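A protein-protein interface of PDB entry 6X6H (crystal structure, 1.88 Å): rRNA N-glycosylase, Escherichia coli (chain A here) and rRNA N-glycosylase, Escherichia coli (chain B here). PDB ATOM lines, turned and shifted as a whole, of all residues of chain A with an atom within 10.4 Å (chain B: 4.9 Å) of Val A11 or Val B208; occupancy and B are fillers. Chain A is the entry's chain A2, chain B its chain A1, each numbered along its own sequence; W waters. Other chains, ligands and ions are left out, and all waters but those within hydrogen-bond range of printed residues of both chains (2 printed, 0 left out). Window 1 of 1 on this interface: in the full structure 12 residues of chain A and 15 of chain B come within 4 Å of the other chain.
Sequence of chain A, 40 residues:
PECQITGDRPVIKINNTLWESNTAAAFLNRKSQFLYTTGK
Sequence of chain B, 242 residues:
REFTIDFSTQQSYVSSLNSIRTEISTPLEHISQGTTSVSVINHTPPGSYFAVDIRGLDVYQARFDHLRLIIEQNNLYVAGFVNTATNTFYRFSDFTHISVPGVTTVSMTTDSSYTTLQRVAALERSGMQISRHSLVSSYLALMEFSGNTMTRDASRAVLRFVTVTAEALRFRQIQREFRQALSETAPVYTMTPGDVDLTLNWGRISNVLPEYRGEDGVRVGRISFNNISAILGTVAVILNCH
NH2 of Arg B204 is in salt-bridge range of OE1 of Glu A20 (2.8 Å). The side-chain hydroxyl (OG1) of Thr A23 lies within hydrogen-bond range of the guanidinium group (NH2) of Arg B204 (3.4 Å).
O of Val A11 lies close to OG of Ser A21 (3.2 Å). OE1 of Glu A20 sits at hydrogen-bond distance from OG1 of Thr A23 (2.6 Å). O of Pro A10 sits at hydrogen-bond distance from N of Ser A21, 3.3 Å away.
Among the printed residues, merely in contact across the chains: Cys A3 with Asn B207, Ile A5 with Arg B204, Pro A10 with Asn B207, Val A11 with Val B208, Val A11 with Glu B211, Leu A18 with Glu B211, Leu A18 with Tyr B212, Leu A18 with Val B218 and Glu A20 with Val B208.
Val A11 touches just these residues of chain B: Val B208 (3.8 Å) and Glu B211 (3.8 Å). Val B208 touches two residues of chain A. No residue of chain A comes within 4 Å of Leu B209. No residue of chain A comes within 4 Å of Pro B210. Glu B211 touches just these residues of chain A: Val A11 (3.8 Å) and Leu A18 (3.7 Å). Printed residues of chain B within 4 Å of Pro A10: Asn B207 (3.7 Å). Of the printed residues of chain A, Val B218 touches Leu A18 (3.3 Å). Of the printed residues of chain B, Leu A18 touches Glu B211 (3.7 Å), Tyr B212 (3.7 Å) and Val B218 (3.3 Å). Printed residues of chain B within 4 Å of Thr A23: Arg B204 (3.4 Å). Of the printed residues of chain B, Ile A5 touches Arg B204 (3.6 Å). Glu A2 touches none of the printed residues of chain B. The nearest residue of chain B that does not touch Val A11 is Asn B207 (4.7 Å). The nearest printed residue of chain A that does not touch Arg B204 is Glu A2 (4.2 Å).
Hydrophobic or aromatic side chains of chain A within 4 Å of the printed part of chain B: Ile A5, Pro A10, Val A11 and Leu A18. Along chain A the printed residues that touch a printed residue of chain B span positions 3 to 23. Of the 11 printed residues of chain B, 6 touch a printed residue of chain A. Among the printed residues, Asp or Glu carboxylates within 4 Å of a Lys or Arg side-chain nitrogen of the other chain: Glu A20 with Arg B204.
Water W1 lies within hydrogen-bond range of the side-chain carboxylate (OE2) of Glu A20 (2.7 Å) and the backbone carbonyl oxygen (O) of Arg B204 (3.0 Å). Water W2 lies within hydrogen-bond range of the backbone carbonyl oxygen of Pro A10 (2.8 Å) and the side-chain amide nitrogen of Asn B207 (2.9 Å).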
ATOM      1  N   GLU A   2     -29.651 -31.444 -15.895  1.00  0.00           N
ATOM      2  CA  GLU A   2     -28.700 -32.394 -16.464  1.00  0.00           C
ATOM      3  C   GLU A   2     -27.574 -31.713 -17.225  1.00  0.00           C
ATOM      4  O   GLU A   2     -26.540 -32.343 -17.466  1.00  0.00           O
ATOM      5  CB  GLU A   2     -29.422 -33.369 -17.393  1.00  0.00           C
ATOM      6  CG  GLU A   2     -30.638 -34.051 -16.784  1.00  0.00           C
ATOM      7  CD  GLU A   2     -31.899 -33.202 -16.845  1.00  0.00           C
ATOM      8  OE1 GLU A   2     -31.832 -31.995 -16.525  1.00  0.00           O
ATOM      9  OE2 GLU A   2     -32.961 -33.743 -17.217  1.00  0.00           O
ATOM     10  N   CYS A   3     -27.745 -30.447 -17.606  1.00  0.00           N
ATOM     11  CA  CYS A   3     -26.764 -29.790 -18.464  1.00  0.00           C
ATOM     12  C   CYS A   3     -25.455 -29.526 -17.730  1.00  0.00           C
ATOM     13  O   CYS A   3     -24.371 -29.629 -18.319  1.00  0.00           O
ATOM     14  CB  CYS A   3     -27.346 -28.484 -18.998  1.00  0.00           C
ATOM     15  SG  CYS A   3     -28.735 -28.691 -20.140  1.00  0.00           S
ATOM     16  N   GLN A   4     -25.531 -29.192 -16.447  1.00  0.00           N
ATOM     17  CA  GLN A   4     -24.392 -28.687 -15.698  1.00  0.00           C
ATOM     18  C   GLN A   4     -23.979 -29.687 -14.630  1.00  0.00           C
ATOM     19  O   GLN A   4     -24.829 -30.215 -13.904  1.00  0.00           O
ATOM     20  CB  GLN A   4     -24.724 -27.342 -15.054  1.00  0.00           C
ATOM     21  CG  GLN A   4     -23.610 -26.755 -14.205  1.00  0.00           C
ATOM     22  CD  GLN A   4     -24.092 -25.561 -13.403  1.00  0.00           C
ATOM     23  OE1 GLN A   4     -25.215 -25.082 -13.593  1.00  0.00           O
ATOM     24  NE2 GLN A   4     -23.251 -25.078 -12.496  1.00  0.00           N
ATOM     25  N   ILE A   5     -22.674 -29.944 -14.540  1.00  0.00           N
ATOM     26  CA  ILE A   5     -22.097 -30.687 -13.425  1.00  0.00           C
ATOM     27  C   ILE A   5     -21.686 -29.682 -12.356  1.00  0.00           C
ATOM     28  O   ILE A   5     -22.285 -29.630 -11.274  1.00  0.00           O
ATOM     29  CB  ILE A   5     -20.897 -31.548 -13.865  1.00  0.00           C
ATOM     30  CG1 ILE A   5     -21.338 -32.640 -14.838  1.00  0.00           C
ATOM     31  CG2 ILE A   5     -20.216 -32.194 -12.658  1.00  0.00           C
ATOM     32  CD1 ILE A   5     -20.229 -33.616 -15.173  1.00  0.00           C
ATOM     33  N   THR A   6     -20.651 -28.892 -12.645  1.00  0.00           N
ATOM     34  CA  THR A   6     -20.197 -27.819 -11.772  1.00  0.00           C
ATOM     35  C   THR A   6     -19.773 -26.629 -12.623  1.00  0.00           C
ATOM     36  O   THR A   6     -19.501 -26.757 -13.819  1.00  0.00           O
ATOM     37  CB  THR A   6     -19.017 -28.238 -10.875  1.00  0.00           C
ATOM     38  OG1 THR A   6     -17.814 -28.272 -11.652  1.00  0.00           O
ATOM     39  CG2 THR A   6     -19.243 -29.603 -10.265  1.00  0.00           C
ATOM     40  N   GLY A   7     -19.700 -25.462 -11.984  1.00  0.00           N
ATOM     41  CA  GLY A   7     -19.229 -24.275 -12.661  1.00  0.00           C
ATOM     42  C   GLY A   7     -20.262 -23.672 -13.593  1.00  0.00           C
ATOM     43  O   GLY A   7     -21.437 -24.042 -13.604  1.00  0.00           O
ATOM     44  N   ASP A   8     -19.798 -22.714 -14.396  1.00  0.00           N
ATOM     45  CA  ASP A   8     -20.693 -21.958 -15.264  1.00  0.00           C
ATOM     46  C   ASP A   8     -20.117 -21.729 -16.657  1.00  0.00           C
ATOM     47  O   ASP A   8     -20.691 -20.948 -17.426  1.00  0.00           O
ATOM     48  CB  ASP A   8     -21.055 -20.601 -14.623  1.00  0.00           C
ATOM     49  CG  ASP A   8     -19.899 -19.599 -14.648  1.00  0.00           C
ATOM     50  OD1 ASP A   8     -18.728 -20.012 -14.769  1.00  0.00           O
ATOM     51  OD2 ASP A   8     -20.160 -18.383 -14.542  1.00  0.00           O
ATOM     52  N   ARG A   9     -19.014 -22.374 -17.009  1.00  0.00           N
ATOM     53  CA  ARG A   9     -18.378 -22.143 -18.299  1.00  0.00           C
ATOM     54  C   ARG A   9     -18.511 -23.394 -19.151  1.00  0.00           C
ATOM     55  O   ARG A   9     -17.800 -24.383 -18.905  1.00  0.00           O
ATOM     56  CB  ARG A   9     -16.905 -21.772 -18.108  1.00  0.00           C
ATOM     57  CG  ARG A   9     -16.138 -21.508 -19.394  1.00  0.00           C
ATOM     58  CD  ARG A   9     -14.658 -21.279 -19.076  1.00  0.00           C
ATOM     59  NE  ARG A   9     -13.905 -20.727 -20.200  1.00  0.00           N
ATOM     60  CZ  ARG A   9     -12.634 -20.331 -20.126  1.00  0.00           C
ATOM     61  NH1 ARG A   9     -11.962 -20.425 -18.978  1.00  0.00           N
ATOM     62  NH2 ARG A   9     -12.030 -19.840 -21.204  1.00  0.00           N
ATOM     63  N   PRO A  10     -19.398 -23.413 -20.149  1.00  0.00           N
ATOM     64  CA  PRO A  10     -19.625 -24.670 -20.886  1.00  0.00           C
ATOM     65  C   PRO A  10     -18.376 -25.229 -21.557  1.00  0.00           C
ATOM     66  O   PRO A  10     -18.100 -26.433 -21.443  1.00  0.00           O
ATOM     67  CB  PRO A  10     -20.704 -24.277 -21.907  1.00  0.00           C
ATOM     68  CG  PRO A  10     -21.423 -23.128 -21.264  1.00  0.00           C
ATOM     69  CD  PRO A  10     -20.370 -22.365 -20.514  1.00  0.00           C
ATOM     70  N   VAL A  11     -17.612 -24.395 -22.267  1.00  0.00           N
ATOM     71  CA  VAL A  11     -16.523 -24.884 -23.107  1.00  0.00           C
ATOM     72  C   VAL A  11     -15.304 -23.979 -22.992  1.00  0.00           C
ATOM     73  O   VAL A  11     -15.387 -22.817 -22.586  1.00  0.00           O
ATOM     74  CB  VAL A  11     -16.925 -25.004 -24.596  1.00  0.00           C
ATOM     75  CG1 VAL A  11     -18.144 -25.914 -24.759  1.00  0.00           C
ATOM     76  CG2 VAL A  11     -17.206 -23.612 -25.177  1.00  0.00           C
ATOM     77  N   ILE A  12     -14.156 -24.553 -23.344  1.00  0.00           N
ATOM     78  CA  ILE A  12     -12.908 -23.824 -23.535  1.00  0.00           C
ATOM     79  C   ILE A  12     -12.362 -24.245 -24.891  1.00  0.00           C
ATOM     80  O   ILE A  12     -12.229 -25.444 -25.162  1.00  0.00           O
ATOM     81  CB  ILE A  12     -11.878 -24.117 -22.427  1.00  0.00           C
ATOM     82  CG1 ILE A  12     -12.440 -23.745 -21.053  1.00  0.00           C
ATOM     83  CG2 ILE A  12     -10.586 -23.357 -22.682  1.00  0.00           C
ATOM     84  CD1 ILE A  12     -11.500 -24.070 -19.899  1.00  0.00           C
ATOM     85  N   LYS A  13     -12.098 -23.270 -25.754  1.00  0.00           N
ATOM     86  CA  LYS A  13     -11.488 -23.536 -27.049  1.00  0.00           C
ATOM     87  C   LYS A  13      -9.973 -23.571 -26.867  1.00  0.00           C
ATOM     88  O   LYS A  13      -9.372 -22.588 -26.417  1.00  0.00           O
ATOM     89  CB  LYS A  13     -11.900 -22.475 -28.065  1.00  0.00           C
ATOM     90  CG  LYS A  13     -11.392 -22.736 -29.472  1.00  0.00           C
ATOM     91  CD  LYS A  13     -11.959 -21.726 -30.452  1.00  0.00           C
ATOM     92  CE  LYS A  13     -11.315 -21.876 -31.817  1.00  0.00           C
ATOM     93  NZ  LYS A  13     -11.759 -20.816 -32.761  1.00  0.00           N
ATOM     94  N   ILE A  14      -9.365 -24.713 -27.174  1.00  0.00           N
ATOM     95  CA  ILE A  14      -7.924 -24.904 -27.032  1.00  0.00           C
ATOM     96  C   ILE A  14      -7.424 -25.450 -28.362  1.00  0.00           C
ATOM     97  O   ILE A  14      -7.795 -26.563 -28.750  1.00  0.00           O
ATOM     98  CB  ILE A  14      -7.568 -25.859 -25.887  1.00  0.00           C
ATOM     99  CG1 ILE A  14      -8.268 -25.453 -24.590  1.00  0.00           C
ATOM    100  CG2 ILE A  14      -6.059 -25.894 -25.666  1.00  0.00           C
ATOM    101  CD1 ILE A  14      -8.002 -26.398 -23.441  1.00  0.00           C
ATOM    102  N   THR A  17      -9.775 -26.842 -30.876  1.00  0.00           N
ATOM    103  CA  THR A  17     -10.568 -27.959 -30.374  1.00  0.00           C
ATOM    104  C   THR A  17     -11.428 -27.471 -29.216  1.00  0.00           C
ATOM    105  O   THR A  17     -10.930 -26.787 -28.318  1.00  0.00           O
ATOM    106  CB  THR A  17      -9.678 -29.131 -29.926  1.00  0.00           C
ATOM    107  OG1 THR A  17      -9.002 -29.679 -31.063  1.00  0.00           O
ATOM    108  CG2 THR A  17     -10.518 -30.225 -29.259  1.00  0.00           C
ATOM    109  N   LEU A  18     -12.707 -27.844 -29.224  1.00  0.00           N
ATOM    110  CA  LEU A  18     -13.655 -27.403 -28.202  1.00  0.00           C
ATOM    111  C   LEU A  18     -13.705 -28.432 -27.072  1.00  0.00           C
ATOM    112  O   LEU A  18     -14.158 -29.562 -27.278  1.00  0.00           O
ATOM    113  CB  LEU A  18     -15.034 -27.208 -28.829  1.00  0.00           C
ATOM    114  CG  LEU A  18     -15.968 -26.210 -28.158  1.00  0.00           C
ATOM    115  CD1 LEU A  18     -15.306 -24.838 -28.118  1.00  0.00           C
ATOM    116  CD2 LEU A  18     -17.294 -26.153 -28.909  1.00  0.00           C
ATOM    117  N   TRP A  19     -13.262 -28.031 -25.877  1.00  0.00           N
ATOM    118  CA  TRP A  19     -13.256 -28.880 -24.692  1.00  0.00           C
ATOM    119  C   TRP A  19     -14.389 -28.504 -23.744  1.00  0.00           C
ATOM    120  O   TRP A  19     -14.610 -27.321 -23.475  1.00  0.00           O
ATOM    121  CB  TRP A  19     -11.944 -28.744 -23.917  1.00  0.00           C
ATOM    122  CG  TRP A  19     -10.767 -29.374 -24.573  1.00  0.00           C
ATOM    123  CD1 TRP A  19      -9.988 -28.843 -25.567  1.00  0.00           C
ATOM    124  CD2 TRP A  19     -10.211 -30.650 -24.259  1.00  0.00           C
ATOM    125  NE1 TRP A  19      -8.982 -29.729 -25.897  1.00  0.00           N
ATOM    126  CE2 TRP A  19      -9.103 -30.846 -25.113  1.00  0.00           C
ATOM    127  CE3 TRP A  19     -10.545 -31.655 -23.345  1.00  0.00           C
ATOM    128  CZ2 TRP A  19      -8.334 -32.004 -25.077  1.00  0.00           C
ATOM    129  CZ3 TRP A  19      -9.778 -32.810 -23.317  1.00  0.00           C
ATOM    130  CH2 TRP A  19      -8.684 -32.971 -24.173  1.00  0.00           C
ATOM    131  N   GLU A  20     -15.069 -29.510 -23.197  1.00  0.00           N
ATOM    132  CA  GLU A  20     -15.836 -29.269 -21.978  1.00  0.00           C
ATOM    133  C   GLU A  20     -14.893 -28.721 -20.910  1.00  0.00           C
ATOM    134  O   GLU A  20     -13.853 -29.322 -20.631  1.00  0.00           O
ATOM    135  CB  GLU A  20     -16.499 -30.556 -21.492  1.00  0.00           C
ATOM    136  CG  GLU A  20     -17.312 -30.355 -20.224  1.00  0.00           C
ATOM    137  CD  GLU A  20     -17.586 -31.652 -19.487  1.00  0.00           C
ATOM    138  OE1 GLU A  20     -16.610 -32.340 -19.119  1.00  0.00           O
ATOM    139  OE2 GLU A  20     -18.774 -31.981 -19.276  1.00  0.00           O
ATOM    140  N   SER A  21     -15.256 -27.574 -20.322  1.00  0.00           N
ATOM    141  CA  SER A  21     -14.332 -26.899 -19.412  1.00  0.00           C
ATOM    142  C   SER A  21     -13.961 -27.798 -18.243  1.00  0.00           C
ATOM    143  O   SER A  21     -12.791 -27.850 -17.838  1.00  0.00           O
ATOM    144  CB  SER A  21     -14.937 -25.588 -18.904  1.00  0.00           C
ATOM    145  OG  SER A  21     -15.284 -24.728 -19.976  1.00  0.00           O
ATOM    146  N   ASN A  22     -14.940 -28.531 -17.704  1.00  0.00           N
ATOM    147  CA  ASN A  22     -14.681 -29.396 -16.559  1.00  0.00           C
ATOM    148  C   ASN A  22     -13.684 -30.505 -16.885  1.00  0.00           C
ATOM    149  O   ASN A  22     -12.914 -30.908 -16.007  1.00  0.00           O
ATOM    150  CB  ASN A  22     -15.992 -29.997 -16.042  1.00  0.00           C
ATOM    151  CG  ASN A  22     -16.782 -29.020 -15.175  1.00  0.00           C
ATOM    152  OD1 ASN A  22     -16.221 -28.097 -14.586  1.00  0.00           O
ATOM    153  ND2 ASN A  22     -18.085 -29.238 -15.076  1.00  0.00           N
ATOM    154  N   THR A  23     -13.675 -31.006 -18.126  1.00  0.00           N
ATOM    155  CA  THR A  23     -12.698 -32.026 -18.495  1.00  0.00           C
ATOM    156  C   THR A  23     -11.286 -31.445 -18.482  1.00  0.00           C
ATOM    157  O   THR A  23     -10.373 -32.026 -17.886  1.00  0.00           O
ATOM    158  CB  THR A  23     -13.029 -32.621 -19.873  1.00  0.00           C
ATOM    159  OG1 THR A  23     -14.308 -33.259 -19.839  1.00  0.00           O
ATOM    160  CG2 THR A  23     -11.980 -33.669 -20.275  1.00  0.00           C
ATOM    161  N   ALA A  24     -11.101 -30.279 -19.104  1.00  0.00           N
ATOM    162  CA  ALA A  24      -9.792 -29.629 -19.096  1.00  0.00           C
ATOM    163  C   ALA A  24      -9.333 -29.314 -17.680  1.00  0.00           C
ATOM    164  O   ALA A  24      -8.166 -29.543 -17.333  1.00  0.00           O
ATOM    165  CB  ALA A  24      -9.826 -28.349 -19.934  1.00  0.00           C
ATOM    166  N   ALA A  25     -10.240 -28.796 -16.841  1.00  0.00           N
ATOM    167  CA  ALA A  25      -9.867 -28.454 -15.472  1.00  0.00           C
ATOM    168  C   ALA A  25      -9.382 -29.666 -14.699  1.00  0.00           C
ATOM    169  O   ALA A  25      -8.517 -29.539 -13.825  1.00  0.00           O
ATOM    170  CB  ALA A  25     -11.055 -27.831 -14.735  1.00  0.00           C
ATOM    171  N   ARG B 204     -23.933 -33.597 -20.443  1.00  0.00           N
ATOM    172  CA  ARG B 204     -22.632 -32.993 -20.734  1.00  0.00           C
ATOM    173  C   ARG B 204     -22.490 -32.684 -22.222  1.00  0.00           C
ATOM    174  O   ARG B 204     -22.045 -31.594 -22.604  1.00  0.00           O
ATOM    175  CB  ARG B 204     -21.505 -33.923 -20.268  1.00  0.00           C
ATOM    176  CG  ARG B 204     -21.427 -34.128 -18.756  1.00  0.00           C
ATOM    177  CD  ARG B 204     -20.424 -35.226 -18.385  1.00  0.00           C
ATOM    178  NE  ARG B 204     -19.034 -34.773 -18.440  1.00  0.00           N
ATOM    179  CZ  ARG B 204     -17.979 -35.579 -18.319  1.00  0.00           C
ATOM    180  NH1 ARG B 204     -18.154 -36.887 -18.145  1.00  0.00           N
ATOM    181  NH2 ARG B 204     -16.749 -35.084 -18.373  1.00  0.00           N
ATOM    182  N   ILE B 205     -22.864 -33.638 -23.078  1.00  0.00           N
ATOM    183  CA  ILE B 205     -22.828 -33.412 -24.524  1.00  0.00           C
ATOM    184  C   ILE B 205     -23.764 -32.274 -24.914  1.00  0.00           C
ATOM    185  O   ILE B 205     -23.419 -31.418 -25.744  1.00  0.00           O
ATOM    186  CB  ILE B 205     -23.185 -34.711 -25.266  1.00  0.00           C
ATOM    187  CG1 ILE B 205     -22.108 -35.770 -25.029  1.00  0.00           C
ATOM    188  CG2 ILE B 205     -23.396 -34.440 -26.765  1.00  0.00           C
ATOM    189  CD1 ILE B 205     -22.543 -37.176 -25.459  1.00  0.00           C
ATOM    190  N   SER B 206     -24.958 -32.239 -24.312  1.00  0.00           N
ATOM    191  CA  SER B 206     -25.936 -31.207 -24.649  1.00  0.00           C
ATOM    192  C   SER B 206     -25.444 -29.814 -24.270  1.00  0.00           C
ATOM    193  O   SER B 206     -25.870 -28.818 -24.870  1.00  0.00           O
ATOM    194  CB  SER B 206     -27.276 -31.500 -23.949  1.00  0.00           C
ATOM    195  OG  SER B 206     -27.824 -32.740 -24.375  1.00  0.00           O
ATOM    196  N   ASN B 207     -24.589 -29.719 -23.254  1.00  0.00           N
ATOM    197  CA  ASN B 207     -24.053 -28.427 -22.837  1.00  0.00           C
ATOM    198  C   ASN B 207     -22.938 -27.928 -23.753  1.00  0.00           C
ATOM    199  O   ASN B 207     -22.699 -26.716 -23.819  1.00  0.00           O
ATOM    200  CB  ASN B 207     -23.529 -28.520 -21.402  1.00  0.00           C
ATOM    201  CG  ASN B 207     -23.605 -27.194 -20.671  1.00  0.00           C
ATOM    202  OD1 ASN B 207     -24.613 -26.492 -20.754  1.00  0.00           O
ATOM    203  ND2 ASN B 207     -22.537 -26.837 -19.960  1.00  0.00           N
ATOM    204  N   VAL B 208     -22.267 -28.823 -24.467  1.00  0.00           N
ATOM    205  CA  VAL B 208     -21.089 -28.475 -25.268  1.00  0.00           C
ATOM    206  C   VAL B 208     -21.447 -28.217 -26.730  1.00  0.00           C
ATOM    207  O   VAL B 208     -21.039 -27.211 -27.309  1.00  0.00           O
ATOM    208  CB  VAL B 208     -20.026 -29.589 -25.127  1.00  0.00           C
ATOM    209  CG1 VAL B 208     -18.853 -29.364 -26.114  1.00  0.00           C
ATOM    210  CG2 VAL B 208     -19.509 -29.624 -23.704  1.00  0.00           C
ATOM    211  N   LEU B 209     -22.213 -29.114 -27.351  1.00  0.00           N
ATOM    212  CA  LEU B 209     -22.455 -28.992 -28.787  1.00  0.00           C
ATOM    213  C   LEU B 209     -23.086 -27.664 -29.230  1.00  0.00           C
ATOM    214  O   LEU B 209     -22.724 -27.198 -30.324  1.00  0.00           O
ATOM    215  CB  LEU B 209     -23.296 -30.184 -29.273  1.00  0.00           C
ATOM    216  CG  LEU B 209     -22.591 -31.546 -29.223  1.00  0.00           C
ATOM    217  CD1 LEU B 209     -23.461 -32.624 -29.886  1.00  0.00           C
ATOM    218  CD2 LEU B 209     -21.200 -31.521 -29.883  1.00  0.00           C
ATOM    219  N   PRO B 210     -23.981 -27.003 -28.481  1.00  0.00           N
ATOM    220  CA  PRO B 210     -24.482 -25.694 -28.959  1.00  0.00           C
ATOM    221  C   PRO B 210     -23.399 -24.634 -29.119  1.00  0.00           C
ATOM    222  O   PRO B 210     -23.636 -23.635 -29.815  1.00  0.00           O
ATOM    223  CB  PRO B 210     -25.499 -25.281 -27.886  1.00  0.00           C
ATOM    224  CG  PRO B 210     -25.959 -26.543 -27.304  1.00  0.00           C
ATOM    225  CD  PRO B 210     -24.751 -27.475 -27.318  1.00  0.00           C
ATOM    226  N   GLU B 211     -22.225 -24.818 -28.517  1.00  0.00           N
ATOM    227  CA  GLU B 211     -21.124 -23.871 -28.653  1.00  0.00           C
ATOM    228  C   GLU B 211     -20.247 -24.134 -29.870  1.00  0.00           C
ATOM    229  O   GLU B 211     -19.356 -23.327 -30.160  1.00  0.00           O
ATOM    230  CB  GLU B 211     -20.246 -23.895 -27.390  1.00  0.00           C
ATOM    231  CG  GLU B 211     -21.046 -23.737 -26.102  1.00  0.00           C
ATOM    232  CD  GLU B 211     -21.850 -22.458 -26.083  1.00  0.00           C
ATOM    233  OE1 GLU B 211     -21.307 -21.410 -26.489  1.00  0.00           O
ATOM    234  OE2 GLU B 211     -23.027 -22.497 -25.672  1.00  0.00           O
ATOM    235  N   TYR B 212     -20.459 -25.241 -30.571  1.00  0.00           N
ATOM    236  CA  TYR B 212     -19.598 -25.599 -31.690  1.00  0.00           C
ATOM    237  C   TYR B 212     -19.766 -24.602 -32.832  1.00  0.00           C
ATOM    238  O   TYR B 212     -20.888 -24.265 -33.219  1.00  0.00           O
ATOM    239  CB  TYR B 212     -19.920 -27.018 -32.158  1.00  0.00           C
ATOM    240  CG  TYR B 212     -19.074 -27.468 -33.331  1.00  0.00           C
ATOM    241  CD1 TYR B 212     -17.795 -27.983 -33.136  1.00  0.00           C
ATOM    242  CD2 TYR B 212     -19.550 -27.368 -34.631  1.00  0.00           C
ATOM    243  CE1 TYR B 212     -17.013 -28.392 -34.221  1.00  0.00           C
ATOM    244  CE2 TYR B 212     -18.776 -27.763 -35.710  1.00  0.00           C
ATOM    245  CZ  TYR B 212     -17.514 -28.283 -35.504  1.00  0.00           C
ATOM    246  OH  TYR B 212     -16.748 -28.671 -36.594  1.00  0.00           O
ATOM    247  N   VAL B 218     -14.184 -31.869 -30.896  1.00  0.00           N
ATOM    248  CA  VAL B 218     -14.937 -31.662 -29.661  1.00  0.00           C
ATOM    249  C   VAL B 218     -14.504 -32.744 -28.674  1.00  0.00           C
ATOM    250  O   VAL B 218     -14.337 -33.912 -29.058  1.00  0.00           O
ATOM    251  CB  VAL B 218     -16.464 -31.716 -29.907  1.00  0.00           C
ATOM    252  CG1 VAL B 218     -17.260 -31.678 -28.599  1.00  0.00           C
ATOM    253  CG2 VAL B 218     -16.915 -30.577 -30.820  1.00  0.00           C
ATOM    254  N   VAL B 220     -15.517 -34.163 -24.758  1.00  0.00           N
ATOM    255  CA  VAL B 220     -16.405 -34.164 -23.594  1.00  0.00           C
ATOM    256  C   VAL B 220     -16.013 -35.383 -22.773  1.00  0.00           C
ATOM    257  O   VAL B 220     -16.370 -36.512 -23.128  1.00  0.00           O
ATOM    258  CB  VAL B 220     -17.890 -34.223 -23.983  1.00  0.00           C
ATOM    259  CG1 VAL B 220     -18.763 -34.101 -22.742  1.00  0.00           C
ATOM    260  CG2 VAL B 220     -18.239 -33.134 -24.988  1.00  0.00           C
HETATM  261  O   HOH W   1     -20.621 -30.344 -20.340  1.00  0.00           O
HETATM  262  O   HOH W   2     -19.898 -27.925 -19.935  1.00  0.00           O
